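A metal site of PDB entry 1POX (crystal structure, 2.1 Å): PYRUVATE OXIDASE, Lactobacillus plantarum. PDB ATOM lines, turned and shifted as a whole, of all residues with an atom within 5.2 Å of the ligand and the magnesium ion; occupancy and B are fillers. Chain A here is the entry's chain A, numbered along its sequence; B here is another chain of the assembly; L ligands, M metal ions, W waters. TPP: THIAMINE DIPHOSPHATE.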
ATOM      1  N   ASN A  84      31.383  18.330  -3.021  1.00  0.00           N
ATOM      2  CA  ASN A  84      30.729  19.608  -3.221  1.00  0.00           C
ATOM      3  C   ASN A  84      31.712  20.730  -3.440  1.00  0.00           C
ATOM      4  O   ASN A  84      31.379  21.692  -4.147  1.00  0.00           O
ATOM      5  CB  ASN A  84      29.826  19.966  -2.046  1.00  0.00           C
ATOM      6  CG  ASN A  84      28.468  19.286  -2.181  1.00  0.00           C
ATOM      7  OD1 ASN A  84      28.358  18.078  -2.424  1.00  0.00           O
ATOM      8  ND2 ASN A  84      27.382  20.028  -2.040  1.00  0.00           N
ATOM      9  N   VAL A 386      24.667  30.626   0.435  1.00  0.00           N
ATOM     10  CA  VAL A 386      23.704  30.520  -0.667  1.00  0.00           C
ATOM     11  C   VAL A 386      22.270  30.529  -0.092  1.00  0.00           C
ATOM     12  O   VAL A 386      21.943  29.706   0.791  1.00  0.00           O
ATOM     13  CB  VAL A 386      23.989  29.207  -1.474  1.00  0.00           C
ATOM     14  CG1 VAL A 386      22.857  28.882  -2.451  1.00  0.00           C
ATOM     15  CG2 VAL A 386      25.258  29.382  -2.284  1.00  0.00           C
ATOM     16  N   GLY A 387      21.407  31.373  -0.650  1.00  0.00           N
ATOM     17  CA  GLY A 387      20.027  31.486  -0.196  1.00  0.00           C
ATOM     18  C   GLY A 387      19.645  32.947  -0.244  1.00  0.00           C
ATOM     19  O   GLY A 387      20.215  33.689  -1.076  1.00  0.00           O
ATOM     20  N   ASP A 388      18.745  33.443   0.622  1.00  0.00           N
ATOM     21  CA  ASP A 388      18.386  34.857   0.610  1.00  0.00           C
ATOM     22  C   ASP A 388      19.572  35.788   0.803  1.00  0.00           C
ATOM     23  O   ASP A 388      19.543  36.905   0.276  1.00  0.00           O
ATOM     24  CB  ASP A 388      17.372  35.163   1.706  1.00  0.00           C
ATOM     25  CG  ASP A 388      15.921  34.871   1.350  1.00  0.00           C
ATOM     26  OD1 ASP A 388      15.588  34.618   0.184  1.00  0.00           O
ATOM     27  OD2 ASP A 388      15.123  34.931   2.270  1.00  0.00           O
ATOM     28  N   ILE A 389      20.649  35.377   1.486  1.00  0.00           N
ATOM     29  CA  ILE A 389      21.839  36.219   1.654  1.00  0.00           C
ATOM     30  C   ILE A 389      22.428  36.655   0.322  1.00  0.00           C
ATOM     31  O   ILE A 389      22.911  37.784   0.254  1.00  0.00           O
ATOM     32  CB  ILE A 389      22.922  35.462   2.571  1.00  0.00           C
ATOM     33  CG1 ILE A 389      23.967  36.510   2.955  1.00  0.00           C
ATOM     34  CG2 ILE A 389      23.588  34.248   1.904  1.00  0.00           C
ATOM     35  CD1 ILE A 389      23.420  37.748   3.694  1.00  0.00           C
ATOM     36  N   ALA A 412      26.374  26.512  -6.877  1.00  0.00           N
ATOM     37  CA  ALA A 412      25.577  27.064  -5.790  1.00  0.00           C
ATOM     38  C   ALA A 412      25.336  26.121  -4.614  1.00  0.00           C
ATOM     39  O   ALA A 412      24.221  25.912  -4.136  1.00  0.00           O
ATOM     40  CB  ALA A 412      24.219  27.530  -6.350  1.00  0.00           C
ATOM     41  N   THR A 413      26.437  25.578  -4.110  1.00  0.00           N
ATOM     42  CA  THR A 413      26.425  24.728  -2.934  1.00  0.00           C
ATOM     43  C   THR A 413      26.356  25.579  -1.675  1.00  0.00           C
ATOM     44  O   THR A 413      27.150  26.500  -1.433  1.00  0.00           O
ATOM     45  CB  THR A 413      27.701  23.763  -2.919  1.00  0.00           C
ATOM     46  OG1 THR A 413      27.492  22.935  -1.760  1.00  0.00           O
ATOM     47  CG2 THR A 413      29.095  24.449  -2.882  1.00  0.00           C
ATOM     48  N   MET A 414      25.362  25.275  -0.844  1.00  0.00           N
ATOM     49  CA  MET A 414      25.260  25.839   0.481  1.00  0.00           C
ATOM     50  C   MET A 414      26.439  25.297   1.286  1.00  0.00           C
ATOM     51  O   MET A 414      27.010  24.233   0.993  1.00  0.00           O
ATOM     52  CB  MET A 414      23.955  25.401   1.176  1.00  0.00           C
ATOM     53  CG  MET A 414      22.711  26.018   0.572  1.00  0.00           C
ATOM     54  SD  MET A 414      21.208  25.177   1.141  1.00  0.00           S
ATOM     55  CE  MET A 414      21.277  25.422   2.900  1.00  0.00           C
ATOM     56  N   GLY A 438      23.050  32.153   5.856  1.00  0.00           N
ATOM     57  CA  GLY A 438      21.730  31.867   6.421  1.00  0.00           C
ATOM     58  C   GLY A 438      21.896  30.738   7.431  1.00  0.00           C
ATOM     59  O   GLY A 438      22.921  30.045   7.470  1.00  0.00           O
ATOM     60  N   ASP A 439      20.901  30.502   8.274  1.00  0.00           N
ATOM     61  CA  ASP A 439      20.933  29.404   9.227  1.00  0.00           C
ATOM     62  C   ASP A 439      20.939  28.025   8.569  1.00  0.00           C
ATOM     63  O   ASP A 439      21.634  27.120   9.055  1.00  0.00           O
ATOM     64  CB  ASP A 439      19.752  29.533  10.183  1.00  0.00           C
ATOM     65  CG  ASP A 439      18.366  29.709   9.602  1.00  0.00           C
ATOM     66  OD1 ASP A 439      18.101  29.801   8.381  1.00  0.00           O
ATOM     67  OD2 ASP A 439      17.478  29.810  10.411  1.00  0.00           O
ATOM     68  N   GLY A 440      20.273  27.778   7.431  1.00  0.00           N
ATOM     69  CA  GLY A 440      20.336  26.479   6.786  1.00  0.00           C
ATOM     70  C   GLY A 440      21.751  26.261   6.230  1.00  0.00           C
ATOM     71  O   GLY A 440      22.304  25.155   6.345  1.00  0.00           O
ATOM     72  N   GLY A 441      22.386  27.256   5.599  1.00  0.00           N
ATOM     73  CA  GLY A 441      23.729  27.124   5.047  1.00  0.00           C
ATOM     74  C   GLY A 441      24.796  27.050   6.116  1.00  0.00           C
ATOM     75  O   GLY A 441      25.729  26.257   5.990  1.00  0.00           O
ATOM     76  N   ALA A 442      24.745  27.840   7.195  1.00  0.00           N
ATOM     77  CA  ALA A 442      25.740  27.771   8.262  1.00  0.00           C
ATOM     78  C   ALA A 442      25.609  26.437   9.004  1.00  0.00           C
ATOM     79  O   ALA A 442      26.657  25.900   9.430  1.00  0.00           O
ATOM     80  CB  ALA A 442      25.578  28.883   9.295  1.00  0.00           C
ATOM     81  N   MET A 444      25.137  23.468   7.763  1.00  0.00           N
ATOM     82  CA  MET A 444      25.754  22.393   7.001  1.00  0.00           C
ATOM     83  C   MET A 444      27.263  22.292   7.229  1.00  0.00           C
ATOM     84  O   MET A 444      27.814  21.199   7.069  1.00  0.00           O
ATOM     85  CB  MET A 444      25.516  22.570   5.498  1.00  0.00           C
ATOM     86  CG  MET A 444      24.103  22.211   5.123  1.00  0.00           C
ATOM     87  SD  MET A 444      23.834  22.222   3.326  1.00  0.00           S
ATOM     88  CE  MET A 444      22.132  21.751   3.266  1.00  0.00           C
ATOM     89  N   PHE A 464      22.066  34.562   9.717  1.00  0.00           N
ATOM     90  CA  PHE A 464      20.750  35.166   9.611  1.00  0.00           C
ATOM     91  C   PHE A 464      19.756  34.063   9.953  1.00  0.00           C
ATOM     92  O   PHE A 464      19.434  33.255   9.075  1.00  0.00           O
ATOM     93  CB  PHE A 464      20.564  35.675   8.158  1.00  0.00           C
ATOM     94  CG  PHE A 464      21.436  36.875   7.819  1.00  0.00           C
ATOM     95  CD1 PHE A 464      22.812  36.726   7.638  1.00  0.00           C
ATOM     96  CD2 PHE A 464      20.864  38.127   7.744  1.00  0.00           C
ATOM     97  CE1 PHE A 464      23.607  37.839   7.386  1.00  0.00           C
ATOM     98  CE2 PHE A 464      21.674  39.236   7.485  1.00  0.00           C
ATOM     99  CZ  PHE A 464      23.035  39.091   7.311  1.00  0.00           C
ATOM    100  N   ASN A 466      16.333  32.761  10.382  1.00  0.00           N
ATOM    101  CA  ASN A 466      14.909  32.951  10.157  1.00  0.00           C
ATOM    102  C   ASN A 466      14.134  31.654  10.455  1.00  0.00           C
ATOM    103  O   ASN A 466      12.907  31.631  10.292  1.00  0.00           O
ATOM    104  CB  ASN A 466      14.586  33.420   8.714  1.00  0.00           C
ATOM    105  CG  ASN A 466      15.227  32.667   7.556  1.00  0.00           C
ATOM    106  OD1 ASN A 466      15.822  31.577   7.680  1.00  0.00           O
ATOM    107  ND2 ASN A 466      15.168  33.232   6.361  1.00  0.00           N
ATOM    108  N   CYS A 467      14.778  30.558  10.890  1.00  0.00           N
ATOM    109  CA  CYS A 467      14.164  29.236  11.111  1.00  0.00           C
ATOM    110  C   CYS A 467      13.426  28.709   9.862  1.00  0.00           C
ATOM    111  O   CYS A 467      12.411  28.002   9.877  1.00  0.00           O
ATOM    112  CB  CYS A 467      13.209  29.276  12.331  1.00  0.00           C
ATOM    113  SG  CYS A 467      14.103  29.467  13.908  1.00  0.00           S
ATOM    114  N   GLN A 468      14.057  29.000   8.728  1.00  0.00           N
ATOM    115  CA  GLN A 468      13.523  28.639   7.418  1.00  0.00           C
ATOM    116  C   GLN A 468      14.632  28.484   6.409  1.00  0.00           C
ATOM    117  O   GLN A 468      15.737  29.087   6.556  1.00  0.00           O
ATOM    118  CB  GLN A 468      12.649  29.699   6.799  1.00  0.00           C
ATOM    119  CG  GLN A 468      11.471  30.173   7.557  1.00  0.00           C
ATOM    120  CD  GLN A 468      10.840  31.374   6.894  1.00  0.00           C
ATOM    121  OE1 GLN A 468       9.750  31.755   7.284  1.00  0.00           O
ATOM    122  NE2 GLN A 468      11.314  32.059   5.875  1.00  0.00           N
ATOM    123  N   TYR A 469      14.267  27.712   5.385  1.00  0.00           N
ATOM    124  CA  TYR A 469      14.999  27.739   4.135  1.00  0.00           C
ATOM    125  C   TYR A 469      14.196  28.825   3.369  1.00  0.00           C
ATOM    126  O   TYR A 469      13.327  28.538   2.545  1.00  0.00           O
ATOM    127  CB  TYR A 469      14.922  26.389   3.361  1.00  0.00           C
ATOM    128  CG  TYR A 469      15.732  25.247   3.976  1.00  0.00           C
ATOM    129  CD1 TYR A 469      17.078  25.420   4.262  1.00  0.00           C
ATOM    130  CD2 TYR A 469      15.105  24.049   4.292  1.00  0.00           C
ATOM    131  CE1 TYR A 469      17.819  24.419   4.868  1.00  0.00           C
ATOM    132  CE2 TYR A 469      15.848  23.027   4.885  1.00  0.00           C
ATOM    133  CZ  TYR A 469      17.193  23.217   5.175  1.00  0.00           C
ATOM    134  OH  TYR A 469      17.922  22.195   5.766  1.00  0.00           O
ATOM    135  N   GLY A 470      14.460  30.113   3.640  1.00  0.00           N
ATOM    136  CA  GLY A 470      13.635  31.196   3.129  1.00  0.00           C
ATOM    137  C   GLY A 470      13.600  31.235   1.597  1.00  0.00           C
ATOM    138  O   GLY A 470      12.515  31.401   1.007  1.00  0.00           O
ATOM    139  N   PHE A 471      14.749  31.083   0.905  1.00  0.00           N
ATOM    140  CA  PHE A 471      14.783  31.093  -0.559  1.00  0.00           C
ATOM    141  C   PHE A 471      13.888  29.978  -1.147  1.00  0.00           C
ATOM    142  O   PHE A 471      13.267  30.200  -2.179  1.00  0.00           O
ATOM    143  CB  PHE A 471      16.256  30.913  -1.024  1.00  0.00           C
ATOM    144  CG  PHE A 471      16.715  31.528  -2.382  1.00  0.00           C
ATOM    145  CD1 PHE A 471      16.841  32.907  -2.542  1.00  0.00           C
ATOM    146  CD2 PHE A 471      17.050  30.719  -3.456  1.00  0.00           C
ATOM    147  CE1 PHE A 471      17.304  33.440  -3.737  1.00  0.00           C
ATOM    148  CE2 PHE A 471      17.506  31.259  -4.655  1.00  0.00           C
ATOM    149  CZ  PHE A 471      17.639  32.619  -4.805  1.00  0.00           C
ATOM    150  N   ILE A 472      13.730  28.799  -0.516  1.00  0.00           N
ATOM    151  CA  ILE A 472      12.888  27.726  -1.073  1.00  0.00           C
ATOM    152  C   ILE A 472      11.407  27.899  -0.706  1.00  0.00           C
ATOM    153  O   ILE A 472      10.492  27.595  -1.505  1.00  0.00           O
ATOM    154  CB  ILE A 472      13.413  26.330  -0.577  1.00  0.00           C
ATOM    155  CG1 ILE A 472      14.908  26.188  -0.891  1.00  0.00           C
ATOM    156  CG2 ILE A 472      12.661  25.188  -1.267  1.00  0.00           C
ATOM    157  CD1 ILE A 472      15.390  26.483  -2.326  1.00  0.00           C
ATOM    158  N   PHE A 489      11.589  25.137  10.124  1.00  0.00           N
ATOM    159  CA  PHE A 489      12.189  24.122  10.962  1.00  0.00           C
ATOM    160  C   PHE A 489      12.581  24.669  12.331  1.00  0.00           C
ATOM    161  O   PHE A 489      12.402  25.875  12.590  1.00  0.00           O
ATOM    162  CB  PHE A 489      13.440  23.555  10.236  1.00  0.00           C
ATOM    163  CG  PHE A 489      14.454  24.543   9.651  1.00  0.00           C
ATOM    164  CD1 PHE A 489      15.180  25.406  10.458  1.00  0.00           C
ATOM    165  CD2 PHE A 489      14.667  24.546   8.283  1.00  0.00           C
ATOM    166  CE1 PHE A 489      16.106  26.262   9.879  1.00  0.00           C
ATOM    167  CE2 PHE A 489      15.583  25.404   7.723  1.00  0.00           C
ATOM    168  CZ  PHE A 489      16.304  26.252   8.515  1.00  0.00           C
ATOM    169  N   ILE B  24      16.102  17.317   1.694  1.00  0.00           N
ATOM    170  CA  ILE B  24      16.098  18.773   1.847  1.00  0.00           C
ATOM    171  C   ILE B  24      15.535  19.297   0.534  1.00  0.00           C
ATOM    172  O   ILE B  24      15.984  18.820  -0.515  1.00  0.00           O
ATOM    173  CB  ILE B  24      17.562  19.297   2.083  1.00  0.00           C
ATOM    174  CG1 ILE B  24      18.019  18.816   3.438  1.00  0.00           C
ATOM    175  CG2 ILE B  24      17.636  20.823   1.945  1.00  0.00           C
ATOM    176  CD1 ILE B  24      19.428  19.332   3.849  1.00  0.00           C
ATOM    177  N   PRO B  25      14.548  20.196   0.490  1.00  0.00           N
ATOM    178  CA  PRO B  25      13.908  20.663  -0.739  1.00  0.00           C
ATOM    179  C   PRO B  25      14.778  21.652  -1.513  1.00  0.00           C
ATOM    180  O   PRO B  25      15.755  22.212  -1.028  1.00  0.00           O
ATOM    181  CB  PRO B  25      12.614  21.266  -0.260  1.00  0.00           C
ATOM    182  CG  PRO B  25      13.032  21.854   1.082  1.00  0.00           C
ATOM    183  CD  PRO B  25      13.880  20.739   1.679  1.00  0.00           C
ATOM    184  N   GLY B  26      14.370  21.898  -2.727  1.00  0.00           N
ATOM    185  CA  GLY B  26      15.030  22.857  -3.584  1.00  0.00           C
ATOM    186  C   GLY B  26      14.067  23.056  -4.719  1.00  0.00           C
ATOM    187  O   GLY B  26      13.164  22.223  -4.941  1.00  0.00           O
ATOM    188  N   GLU B  51      22.245  16.673   3.550  1.00  0.00           N
ATOM    189  CA  GLU B  51      21.722  15.528   2.806  1.00  0.00           C
ATOM    190  C   GLU B  51      22.520  14.238   2.954  1.00  0.00           C
ATOM    191  O   GLU B  51      21.939  13.162   2.715  1.00  0.00           O
ATOM    192  CB  GLU B  51      21.593  15.795   1.297  1.00  0.00           C
ATOM    193  CG  GLU B  51      20.728  16.951   0.869  1.00  0.00           C
ATOM    194  CD  GLU B  51      21.413  18.312   0.796  1.00  0.00           C
ATOM    195  OE1 GLU B  51      22.501  18.507   1.337  1.00  0.00           O
ATOM    196  OE2 GLU B  51      20.830  19.221   0.235  1.00  0.00           O
ATOM    197  N   SER B  74      18.256  17.809  -4.024  1.00  0.00           N
ATOM    198  CA  SER B  74      17.974  18.696  -5.135  1.00  0.00           C
ATOM    199  C   SER B  74      19.140  18.651  -6.133  1.00  0.00           C
ATOM    200  O   SER B  74      20.196  18.058  -5.857  1.00  0.00           O
ATOM    201  CB  SER B  74      17.742  20.115  -4.595  1.00  0.00           C
ATOM    202  OG  SER B  74      18.822  20.525  -3.744  1.00  0.00           O
ATOM    203  N   PRO B  77      24.408  20.314  -5.960  1.00  0.00           N
ATOM    204  CA  PRO B  77      24.921  20.074  -4.633  1.00  0.00           C
ATOM    205  C   PRO B  77      24.039  19.268  -3.669  1.00  0.00           C
ATOM    206  O   PRO B  77      24.567  18.710  -2.702  1.00  0.00           O
ATOM    207  CB  PRO B  77      25.255  21.487  -4.200  1.00  0.00           C
ATOM    208  CG  PRO B  77      24.187  22.333  -4.822  1.00  0.00           C
ATOM    209  CD  PRO B  77      24.189  21.742  -6.204  1.00  0.00           C
ATOM    210  N   GLY B  78      22.720  19.193  -3.842  1.00  0.00           N
ATOM    211  CA  GLY B  78      21.870  18.379  -2.992  1.00  0.00           C
ATOM    212  C   GLY B  78      22.202  16.914  -3.195  1.00  0.00           C
ATOM    213  O   GLY B  78      22.483  16.163  -2.261  1.00  0.00           O
ATOM    214  N   HIS B  81      25.861  15.690  -2.127  1.00  0.00           N
ATOM    215  CA  HIS B  81      25.953  15.553  -0.697  1.00  0.00           C
ATOM    216  C   HIS B  81      25.541  14.160  -0.246  1.00  0.00           C
ATOM    217  O   HIS B  81      25.930  13.741   0.846  1.00  0.00           O
ATOM    218  CB  HIS B  81      25.061  16.549   0.086  1.00  0.00           C
ATOM    219  CG  HIS B  81      25.749  17.798   0.626  1.00  0.00           C
ATOM    220  ND1 HIS B  81      25.224  18.898   1.155  1.00  0.00           N
ATOM    221  CD2 HIS B  81      27.107  17.996   0.634  1.00  0.00           C
ATOM    222  CE1 HIS B  81      26.177  19.733   1.472  1.00  0.00           C
ATOM    223  NE2 HIS B  81      27.307  19.182   1.146  1.00  0.00           N
ATOM    224  N   GLN B 114      22.457  25.950 -12.078  1.00  0.00           N
ATOM    225  CA  GLN B 114      22.596  24.681 -11.374  1.00  0.00           C
ATOM    226  C   GLN B 114      22.106  23.486 -12.202  1.00  0.00           C
ATOM    227  O   GLN B 114      21.501  22.533 -11.676  1.00  0.00           O
ATOM    228  CB  GLN B 114      21.826  24.834 -10.047  1.00  0.00           C
ATOM    229  CG  GLN B 114      22.277  23.959  -8.918  1.00  0.00           C
ATOM    230  CD  GLN B 114      21.588  24.380  -7.641  1.00  0.00           C
ATOM    231  OE1 GLN B 114      20.382  24.589  -7.587  1.00  0.00           O
ATOM    232  NE2 GLN B 114      22.320  24.609  -6.563  1.00  0.00           N
HETATM  233  N1' TPP L   1      21.307  21.643  -0.765  1.00  0.00           N
HETATM  234  C2' TPP L   1      22.509  22.142  -1.046  1.00  0.00           C
HETATM  235  CM2 TPP L   1      23.772  21.507  -0.475  1.00  0.00           C
HETATM  236  N3' TPP L   1      22.637  23.217  -1.821  1.00  0.00           N
HETATM  237  C4' TPP L   1      21.555  23.837  -2.359  1.00  0.00           C
HETATM  238  N4' TPP L   1      21.764  24.906  -3.153  1.00  0.00           N
HETATM  239  C5' TPP L   1      20.269  23.369  -1.993  1.00  0.00           C
HETATM  240  C6' TPP L   1      20.183  22.217  -1.209  1.00  0.00           C
HETATM  241  C7' TPP L   1      18.972  24.072  -2.423  1.00  0.00           C
HETATM  242  N3  TPP L   1      18.831  25.372  -1.723  1.00  0.00           N
HETATM  243  C2  TPP L   1      19.165  26.471  -2.346  1.00  0.00           C
HETATM  244  S1  TPP L   1      18.869  27.900  -1.361  1.00  0.00           S
HETATM  245  C5  TPP L   1      18.344  26.825  -0.062  1.00  0.00           C
HETATM  246  C4  TPP L   1      18.372  25.544  -0.473  1.00  0.00           C
HETATM  247  CM4 TPP L   1      17.920  24.413   0.416  1.00  0.00           C
HETATM  248  C6  TPP L   1      17.895  27.315   1.283  1.00  0.00           C
HETATM  249  C7  TPP L   1      18.864  28.321   1.900  1.00  0.00           C
HETATM  250  O7  TPP L   1      18.535  28.366   3.385  1.00  0.00           O
HETATM  251  PA  TPP L   1      19.198  29.329   4.382  1.00  0.00           P
HETATM  252  O1A TPP L   1      18.510  29.202   5.675  1.00  0.00           O
HETATM  253  O2A TPP L   1      20.632  29.120   4.383  1.00  0.00           O
HETATM  254  O3A TPP L   1      18.863  30.777   3.811  1.00  0.00           O
HETATM  255  PB  TPP L   1      17.594  31.765   3.796  1.00  0.00           P
HETATM  256  O1B TPP L   1      17.067  31.716   2.449  1.00  0.00           O
HETATM  257  O2B TPP L   1      18.233  33.025   4.134  1.00  0.00           O
HETATM  258  O3B TPP L   1      16.697  31.267   4.879  1.00  0.00           O
HETATM  259 MG    MG M   1      17.253  30.425   6.667  1.00  0.00          MG
HETATM  260  O   HOH W   1      20.476  26.280  -5.242  1.00  0.00           O
HETATM  261  O   HOH W   2      18.041  35.617   5.248  1.00  0.00           O
HETATM  262  O   HOH W   3      20.804  32.999   3.202  1.00  0.00           O
HETATM  263  O   HOH W   4      19.709  28.932  -4.394  1.00  0.00           O
HETATM  264  O   HOH W   5      20.307  22.339  -5.116  1.00  0.00           O
HETATM  265  O   HOH W   6      18.355  32.097   6.840  1.00  0.00           O
HETATM  266  O   HOH W   7      22.664  30.618   3.362  1.00  0.00           O
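The backbone NH (N) of Asp 439 is in hydrogen-bond range of the backbone carbonyl oxygen (O) of Phe 464 (3.2 Å).
OE1 of Glu 51 of chain B lies within hydrogen-bond range of ND1 of His 81 of chain B, 2.8 Å away.
A ring nitrogen (NE2) of His 81 of chain B is in hydrogen-bond range of the side-chain amide nitrogen (ND2) of Asn 84.
O of Pro 77 of chain B is in hydrogen-bond range of ND2 of Asn 84.
N of Cys 467 lies within hydrogen-bond range of OD2 of Asp 439.
The backbone carbonyl oxygen (O) of Ala 412 is in hydrogen-bond range of the side-chain amide nitrogen (NE2) of Gln 114 of chain B, at 3.3 Å.
Water W6 lies within hydrogen-bond range of O of Phe 464 (2.7 Å), O2B of the ligand (2.9 Å), N of Asp 439 (3.3 Å) and ND2 of Asn 466 (3.4 Å).
Water W7 lies within hydrogen-bond range of O2A of the ligand (2.7 Å), O of Val 386 (2.8 Å) and N of Gly 438 (3.0 Å).
Water W3 lies within hydrogen-bond range of an oxygen (O2B) of the ligand (2.7 Å), the backbone NH (N) of Ile 389 (2.9 Å) and the backbone NH (N) of Asp 388 (3.3 Å).
Water W1 lies within hydrogen-bond range of N4' of the ligand (2.8 Å) and NE2 of Gln 114 of chain B (2.8 Å).
Water W5 bridges OG of Ser 74 of chain B (2.7 Å) and OE1 of Gln 114 of chain B (3.3 Å).
Water W6 is bound to the magnesium ion, at 2.0 Å.
The side-chain carboxylate (OD1) of Asp 439 is bound to the magnesium ion (2.0 Å).
O1A of the ligand is bound to the magnesium ion, at 2.0 Å.
O of Gln 468 binds the magnesium ion, at 2.0 Å.
O3B of the ligand is bound to the magnesium ion (2.1 Å).
The magnesium ion is bound by OD1 of Asn 466 (2.1 Å).
The magnesium ion has six donor atoms within binding distance.
N3 of the ligand sits close to SD of Met 414 (3.7 Å).
Merely in contact with the ligand: Val 386 (3.6 Å), Gly 387 (3.9 Å), Gly 438 (3.6 Å), Met 444 (3.9 Å), Tyr 469 (3.4 Å), Ile 472 (3.5 Å), Ile 24 of chain B (3.9 Å), Pro 25 of chain B (3.4 Å), Ser 74 of chain B (3.3 Å), Pro 77 of chain B (3.5 Å), Gly 78 of chain B (3.99 Å) and His 81 of chain B (3.4 Å).
Hydrophobic or aromatic side chains within 4 Å of the ligand: Met 414, Met 444, Tyr 469, Phe 471, Ile 472, Ile 24 of chain B, Pro 77 of chain B and His 81 of chain B.
The nearest printed residue that does not touch the ligand is Thr 413 (4.2 Å).
The backbone NH (N) of Gly 440 sits at hydrogen-bond distance from an oxygen (O2A) of the ligand, 3.3 Å away.
O of Ala 412 sits at hydrogen-bond distance from N4' of the ligand (2.8 Å).
The backbone NH of Gly 441 sits at hydrogen-bond distance from an oxygen (O2A) of the ligand (2.8 Å).
An oxygen (O1B) of the ligand lies within hydrogen-bond range of the backbone NH (N) of Asp 388 (3.0 Å).
OE2 of Glu 51 of chain B is in hydrogen-bond range of N1' of the ligand, at 2.7 Å.
An oxygen (O1B) of the ligand is in hydrogen-bond range of the backbone NH (N) of Phe 471 (2.9 Å).
The side-chain amide nitrogen of Gln 114 of chain B sits close to a nitrogen (N4') of the ligand.
The backbone NH (N) of Gly 470 sits at hydrogen-bond distance from an oxygen (O1B) of the ligand, at 3.3 Å.
Within 4 Å of the magnesium ion: Asp 439, Asn 466 and Gln 468.
The nearest printed residue that does not touch the magnesium ion is Gly 440 (4.1 Å).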
